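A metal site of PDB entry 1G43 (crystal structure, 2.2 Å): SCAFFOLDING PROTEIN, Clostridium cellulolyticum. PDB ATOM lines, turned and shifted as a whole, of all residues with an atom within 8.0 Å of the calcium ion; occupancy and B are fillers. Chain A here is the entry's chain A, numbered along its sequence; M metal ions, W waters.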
ATOM      1  N   ALA A  17       0.343 -19.897   0.256  1.00  0.00           N
ATOM      2  CA  ALA A  17      -0.797 -19.521  -0.584  1.00  0.00           C
ATOM      3  C   ALA A  17      -0.442 -18.360  -1.512  1.00  0.00           C
ATOM      4  O   ALA A  17      -0.837 -18.332  -2.679  1.00  0.00           O
ATOM      5  CB  ALA A  17      -1.981 -19.135   0.301  1.00  0.00           C
ATOM      6  N   ILE A  22       5.100 -21.397  -8.494  1.00  0.00           N
ATOM      7  CA  ILE A  22       4.143 -22.451  -8.279  1.00  0.00           C
ATOM      8  C   ILE A  22       4.986 -23.708  -8.500  1.00  0.00           C
ATOM      9  O   ILE A  22       5.666 -23.833  -9.525  1.00  0.00           O
ATOM     10  CB  ILE A  22       2.957 -22.329  -9.264  1.00  0.00           C
ATOM     11  CG1 ILE A  22       2.307 -20.959  -9.033  1.00  0.00           C
ATOM     12  CG2 ILE A  22       1.997 -23.502  -9.102  1.00  0.00           C
ATOM     13  CD1 ILE A  22       0.844 -20.760  -9.499  1.00  0.00           C
ATOM     14  N   TYR A  46      -4.159 -27.525 -12.828  1.00  0.00           N
ATOM     15  CA  TYR A  46      -5.111 -26.432 -13.041  1.00  0.00           C
ATOM     16  C   TYR A  46      -5.047 -25.258 -12.057  1.00  0.00           C
ATOM     17  O   TYR A  46      -4.966 -25.457 -10.856  1.00  0.00           O
ATOM     18  CB  TYR A  46      -6.510 -27.020 -13.093  1.00  0.00           C
ATOM     19  CG  TYR A  46      -6.742 -27.940 -14.285  1.00  0.00           C
ATOM     20  CD1 TYR A  46      -6.290 -29.266 -14.300  1.00  0.00           C
ATOM     21  CD2 TYR A  46      -7.420 -27.478 -15.404  1.00  0.00           C
ATOM     22  CE1 TYR A  46      -6.511 -30.106 -15.392  1.00  0.00           C
ATOM     23  CE2 TYR A  46      -7.645 -28.285 -16.503  1.00  0.00           C
ATOM     24  CZ  TYR A  46      -7.198 -29.607 -16.495  1.00  0.00           C
ATOM     25  OH  TYR A  46      -7.459 -30.405 -17.592  1.00  0.00           O
ATOM     26  N   TYR A  47      -5.093 -24.030 -12.563  1.00  0.00           N
ATOM     27  CA  TYR A  47      -4.997 -22.855 -11.695  1.00  0.00           C
ATOM     28  C   TYR A  47      -5.697 -21.627 -12.240  1.00  0.00           C
ATOM     29  O   TYR A  47      -6.194 -21.627 -13.377  1.00  0.00           O
ATOM     30  CB  TYR A  47      -3.530 -22.477 -11.494  1.00  0.00           C
ATOM     31  CG  TYR A  47      -2.825 -22.092 -12.796  1.00  0.00           C
ATOM     32  CD1 TYR A  47      -2.512 -23.057 -13.736  1.00  0.00           C
ATOM     33  CD2 TYR A  47      -2.499 -20.767 -13.077  1.00  0.00           C
ATOM     34  CE1 TYR A  47      -1.873 -22.735 -14.929  1.00  0.00           C
ATOM     35  CE2 TYR A  47      -1.859 -20.423 -14.277  1.00  0.00           C
ATOM     36  CZ  TYR A  47      -1.549 -21.424 -15.199  1.00  0.00           C
ATOM     37  OH  TYR A  47      -0.873 -21.173 -16.356  1.00  0.00           O
ATOM     38  N   THR A  48      -5.755 -20.570 -11.407  1.00  0.00           N
ATOM     39  CA  THR A  48      -6.325 -19.301 -11.833  1.00  0.00           C
ATOM     40  C   THR A  48      -5.151 -18.364 -12.024  1.00  0.00           C
ATOM     41  O   THR A  48      -4.327 -18.157 -11.133  1.00  0.00           O
ATOM     42  CB  THR A  48      -7.358 -18.698 -10.829  1.00  0.00           C
ATOM     43  OG1 THR A  48      -6.878 -18.786  -9.484  1.00  0.00           O
ATOM     44  CG2 THR A  48      -8.728 -19.408 -10.976  1.00  0.00           C
ATOM     45  N   GLN A  49      -5.070 -17.834 -13.227  1.00  0.00           N
ATOM     46  CA  GLN A  49      -4.003 -16.947 -13.662  1.00  0.00           C
ATOM     47  C   GLN A  49      -3.812 -15.682 -12.773  1.00  0.00           C
ATOM     48  O   GLN A  49      -2.701 -15.252 -12.547  1.00  0.00           O
ATOM     49  CB  GLN A  49      -4.324 -16.564 -15.105  1.00  0.00           C
ATOM     50  CG  GLN A  49      -3.145 -16.104 -15.901  1.00  0.00           C
ATOM     51  CD  GLN A  49      -3.481 -15.903 -17.367  1.00  0.00           C
ATOM     52  OE1 GLN A  49      -4.386 -15.139 -17.731  1.00  0.00           O
ATOM     53  NE2 GLN A  49      -2.737 -16.573 -18.231  1.00  0.00           N
ATOM     54  N   ASP A  50      -4.910 -15.135 -12.292  1.00  0.00           N
ATOM     55  CA  ASP A  50      -4.925 -13.911 -11.478  1.00  0.00           C
ATOM     56  C   ASP A  50      -4.482 -12.676 -12.311  1.00  0.00           C
ATOM     57  O   ASP A  50      -5.027 -11.610 -12.152  1.00  0.00           O
ATOM     58  CB  ASP A  50      -4.056 -14.048 -10.232  1.00  0.00           C
ATOM     59  CG  ASP A  50      -4.379 -15.288  -9.449  1.00  0.00           C
ATOM     60  OD1 ASP A  50      -5.546 -15.708  -9.435  1.00  0.00           O
ATOM     61  OD2 ASP A  50      -3.452 -15.836  -8.841  1.00  0.00           O
ATOM     62  N   ALA A  51      -3.481 -12.825 -13.179  1.00  0.00           N
ATOM     63  CA  ALA A  51      -3.039 -11.741 -14.057  1.00  0.00           C
ATOM     64  C   ALA A  51      -2.533 -12.381 -15.358  1.00  0.00           C
ATOM     65  O   ALA A  51      -2.053 -13.508 -15.364  1.00  0.00           O
ATOM     66  CB  ALA A  51      -1.913 -10.909 -13.408  1.00  0.00           C
ATOM     67  N   ASN A  90     -12.146 -21.446 -10.102  1.00  0.00           N
ATOM     68  CA  ASN A  90     -10.801 -21.780  -9.684  1.00  0.00           C
ATOM     69  C   ASN A  90      -9.929 -22.436 -10.736  1.00  0.00           C
ATOM     70  O   ASN A  90      -8.898 -23.035 -10.409  1.00  0.00           O
ATOM     71  CB  ASN A  90     -10.837 -22.608  -8.408  1.00  0.00           C
ATOM     72  CG  ASN A  90     -11.257 -21.774  -7.244  1.00  0.00           C
ATOM     73  OD1 ASN A  90     -11.297 -22.225  -6.101  1.00  0.00           O
ATOM     74  ND2 ASN A  90     -11.597 -20.535  -7.527  1.00  0.00           N
ATOM     75  N   ALA A  91     -10.321 -22.305 -11.990  1.00  0.00           N
ATOM     76  CA  ALA A  91      -9.547 -22.885 -13.055  1.00  0.00           C
ATOM     77  C   ALA A  91      -9.757 -22.204 -14.413  1.00  0.00           C
ATOM     78  O   ALA A  91     -10.727 -22.518 -15.107  1.00  0.00           O
ATOM     79  CB  ALA A  91      -9.846 -24.371 -13.157  1.00  0.00           C
ATOM     80  N   ASP A  92      -8.882 -21.262 -14.791  1.00  0.00           N
ATOM     81  CA  ASP A  92      -8.998 -20.646 -16.101  1.00  0.00           C
ATOM     82  C   ASP A  92      -7.834 -21.010 -17.030  1.00  0.00           C
ATOM     83  O   ASP A  92      -7.858 -20.679 -18.206  1.00  0.00           O
ATOM     84  CB  ASP A  92      -9.166 -19.114 -16.021  1.00  0.00           C
ATOM     85  CG  ASP A  92      -8.120 -18.434 -15.160  1.00  0.00           C
ATOM     86  OD1 ASP A  92      -6.918 -18.675 -15.341  1.00  0.00           O
ATOM     87  OD2 ASP A  92      -8.497 -17.632 -14.309  1.00  0.00           O
ATOM     88  N   ARG A 120       6.088 -15.921 -12.948  1.00  0.00           N
ATOM     89  CA  ARG A 120       5.915 -14.875 -13.936  1.00  0.00           C
ATOM     90  C   ARG A 120       7.282 -14.273 -14.167  1.00  0.00           C
ATOM     91  O   ARG A 120       8.163 -14.321 -13.297  1.00  0.00           O
ATOM     92  CB  ARG A 120       4.966 -13.785 -13.421  1.00  0.00           C
ATOM     93  CG  ARG A 120       3.541 -14.228 -13.219  1.00  0.00           C
ATOM     94  CD  ARG A 120       2.835 -13.224 -12.359  1.00  0.00           C
ATOM     95  NE  ARG A 120       1.481 -13.631 -12.061  1.00  0.00           N
ATOM     96  CZ  ARG A 120       0.719 -13.066 -11.127  1.00  0.00           C
ATOM     97  NH1 ARG A 120       1.200 -12.067 -10.422  1.00  0.00           N
ATOM     98  NH2 ARG A 120      -0.516 -13.504 -10.913  1.00  0.00           N
ATOM     99  N   ASN A 125       3.600 -12.021  -7.219  1.00  0.00           N
ATOM    100  CA  ASN A 125       2.906 -13.067  -6.508  1.00  0.00           C
ATOM    101  C   ASN A 125       1.623 -13.567  -7.150  1.00  0.00           C
ATOM    102  O   ASN A 125       0.871 -12.792  -7.699  1.00  0.00           O
ATOM    103  CB  ASN A 125       2.557 -12.581  -5.094  1.00  0.00           C
ATOM    104  CG  ASN A 125       3.701 -12.753  -4.089  1.00  0.00           C
ATOM    105  OD1 ASN A 125       4.878 -12.797  -4.444  1.00  0.00           O
ATOM    106  ND2 ASN A 125       3.331 -12.844  -2.815  1.00  0.00           N
ATOM    107  N   PHE A 126       1.413 -14.880  -7.065  1.00  0.00           N
ATOM    108  CA  PHE A 126       0.209 -15.524  -7.545  1.00  0.00           C
ATOM    109  C   PHE A 126      -0.605 -15.641  -6.266  1.00  0.00           C
ATOM    110  O   PHE A 126      -0.093 -15.361  -5.172  1.00  0.00           O
ATOM    111  CB  PHE A 126       0.441 -16.985  -7.997  1.00  0.00           C
ATOM    112  CG  PHE A 126       1.171 -17.136  -9.304  1.00  0.00           C
ATOM    113  CD1 PHE A 126       2.512 -17.448  -9.326  1.00  0.00           C
ATOM    114  CD2 PHE A 126       0.477 -17.056 -10.517  1.00  0.00           C
ATOM    115  CE1 PHE A 126       3.161 -17.688 -10.531  1.00  0.00           C
ATOM    116  CE2 PHE A 126       1.135 -17.292 -11.724  1.00  0.00           C
ATOM    117  CZ  PHE A 126       2.470 -17.609 -11.734  1.00  0.00           C
ATOM    118  N   ASP A 127      -1.854 -16.047  -6.403  1.00  0.00           N
ATOM    119  CA  ASP A 127      -2.741 -16.296  -5.282  1.00  0.00           C
ATOM    120  C   ASP A 127      -3.086 -17.754  -5.546  1.00  0.00           C
ATOM    121  O   ASP A 127      -3.921 -18.062  -6.379  1.00  0.00           O
ATOM    122  CB  ASP A 127      -3.993 -15.412  -5.353  1.00  0.00           C
ATOM    123  CG  ASP A 127      -5.068 -15.804  -4.300  1.00  0.00           C
ATOM    124  OD1 ASP A 127      -4.832 -16.676  -3.443  1.00  0.00           O
ATOM    125  OD2 ASP A 127      -6.163 -15.205  -4.353  1.00  0.00           O
ATOM    126  N   GLN A 128      -2.412 -18.656  -4.856  1.00  0.00           N
ATOM    127  CA  GLN A 128      -2.678 -20.055  -5.077  1.00  0.00           C
ATOM    128  C   GLN A 128      -3.967 -20.528  -4.448  1.00  0.00           C
ATOM    129  O   GLN A 128      -4.494 -21.564  -4.825  1.00  0.00           O
ATOM    130  CB  GLN A 128      -1.546 -20.891  -4.520  1.00  0.00           C
ATOM    131  CG  GLN A 128      -0.209 -20.531  -5.091  1.00  0.00           C
ATOM    132  CD  GLN A 128       0.727 -21.694  -4.986  1.00  0.00           C
ATOM    133  OE1 GLN A 128       0.727 -22.562  -5.846  1.00  0.00           O
ATOM    134  NE2 GLN A 128       1.510 -21.745  -3.883  1.00  0.00           N
ATOM    135  N   SER A 129      -4.488 -19.739  -3.498  1.00  0.00           N
ATOM    136  CA  SER A 129      -5.686 -20.164  -2.799  1.00  0.00           C
ATOM    137  C   SER A 129      -6.907 -20.331  -3.673  1.00  0.00           C
ATOM    138  O   SER A 129      -7.845 -20.991  -3.259  1.00  0.00           O
ATOM    139  CB  SER A 129      -5.996 -19.253  -1.579  1.00  0.00           C
ATOM    140  OG  SER A 129      -6.653 -18.032  -1.908  1.00  0.00           O
ATOM    141  N   ASN A 130      -6.913 -19.737  -4.862  1.00  0.00           N
ATOM    142  CA  ASN A 130      -8.065 -19.930  -5.760  1.00  0.00           C
ATOM    143  C   ASN A 130      -7.661 -20.768  -6.982  1.00  0.00           C
ATOM    144  O   ASN A 130      -8.164 -20.584  -8.090  1.00  0.00           O
ATOM    145  CB  ASN A 130      -8.660 -18.589  -6.214  1.00  0.00           C
ATOM    146  CG  ASN A 130      -7.640 -17.711  -6.899  1.00  0.00           C
ATOM    147  OD1 ASN A 130      -6.507 -18.089  -7.039  1.00  0.00           O
ATOM    148  ND2 ASN A 130      -8.060 -16.522  -7.329  1.00  0.00           N
ATOM    149  N   ASP A 131      -6.718 -21.675  -6.750  1.00  0.00           N
ATOM    150  CA  ASP A 131      -6.228 -22.603  -7.755  1.00  0.00           C
ATOM    151  C   ASP A 131      -6.811 -23.987  -7.481  1.00  0.00           C
ATOM    152  O   ASP A 131      -6.652 -24.575  -6.404  1.00  0.00           O
ATOM    153  CB  ASP A 131      -4.705 -22.679  -7.762  1.00  0.00           C
ATOM    154  CG  ASP A 131      -4.073 -21.393  -8.219  1.00  0.00           C
ATOM    155  OD1 ASP A 131      -4.794 -20.512  -8.716  1.00  0.00           O
ATOM    156  OD2 ASP A 131      -2.845 -21.259  -8.089  1.00  0.00           O
ATOM    157  N   TRP A 132      -7.490 -24.488  -8.488  1.00  0.00           N
ATOM    158  CA  TRP A 132      -8.135 -25.780  -8.460  1.00  0.00           C
ATOM    159  C   TRP A 132      -7.215 -26.915  -8.030  1.00  0.00           C
ATOM    160  O   TRP A 132      -7.598 -27.733  -7.209  1.00  0.00           O
ATOM    161  CB  TRP A 132      -8.706 -26.066  -9.841  1.00  0.00           C
ATOM    162  CG  TRP A 132      -9.722 -27.112  -9.818  1.00  0.00           C
ATOM    163  CD1 TRP A 132     -11.049 -26.969  -9.509  1.00  0.00           C
ATOM    164  CD2 TRP A 132      -9.518 -28.509 -10.097  1.00  0.00           C
ATOM    165  NE1 TRP A 132     -11.682 -28.185  -9.573  1.00  0.00           N
ATOM    166  CE2 TRP A 132     -10.768 -29.147  -9.927  1.00  0.00           C
ATOM    167  CE3 TRP A 132      -8.405 -29.276 -10.466  1.00  0.00           C
ATOM    168  CZ2 TRP A 132     -10.926 -30.517 -10.118  1.00  0.00           C
ATOM    169  CZ3 TRP A 132      -8.569 -30.628 -10.653  1.00  0.00           C
ATOM    170  CH2 TRP A 132      -9.816 -31.235 -10.471  1.00  0.00           C
ATOM    171  N   TYR A 134      -4.522 -26.700  -6.301  1.00  0.00           N
ATOM    172  CA  TYR A 134      -3.684 -26.367  -5.160  1.00  0.00           C
ATOM    173  C   TYR A 134      -4.036 -26.916  -3.808  1.00  0.00           C
ATOM    174  O   TYR A 134      -5.175 -26.899  -3.361  1.00  0.00           O
ATOM    175  CB  TYR A 134      -3.518 -24.832  -5.031  1.00  0.00           C
ATOM    176  CG  TYR A 134      -2.680 -24.408  -3.808  1.00  0.00           C
ATOM    177  CD1 TYR A 134      -1.299 -24.588  -3.789  1.00  0.00           C
ATOM    178  CD2 TYR A 134      -3.295 -23.913  -2.654  1.00  0.00           C
ATOM    179  CE1 TYR A 134      -0.539 -24.295  -2.626  1.00  0.00           C
ATOM    180  CE2 TYR A 134      -2.542 -23.624  -1.480  1.00  0.00           C
ATOM    181  CZ  TYR A 134      -1.173 -23.815  -1.479  1.00  0.00           C
ATOM    182  OH  TYR A 134      -0.444 -23.557  -0.351  1.00  0.00           O
HETATM  183 CA    CA M   1      -4.705 -18.019  -8.749  1.00  0.00          CA
HETATM  184  O   HOH W   1      -2.113 -18.949  -8.971  1.00  0.00           O
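Within 4 Å of the calcium ion: Thr 48, Asp 50, Asp 127, Asn 130 and Asp 131. Along chain A the residues within 4 Å of the calcium ion span positions 48 to 131. The nearest printed residue that does not touch the calcium ion is Gln 49 (4.5 Å).
ND2 of Asn 90 sits close to O of Asn 130 (3.5 Å). The side-chain hydroxyl of Ser 129 lies within hydrogen-bond range of the side-chain carboxylate of Asp 127.
The calcium ion is bound by O of Thr 48 (2.4 Å), OG1 of Thr 48 (2.4 Å), OD1 of Asn 130 (2.5 Å), OD1 of Asp 131 (2.5 Å), O of Asp 127 (2.5 Å), OD2 of Asp 50 (2.5 Å), OD1 of Asp 50 (2.6 Å) and water W1 (2.8 Å).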
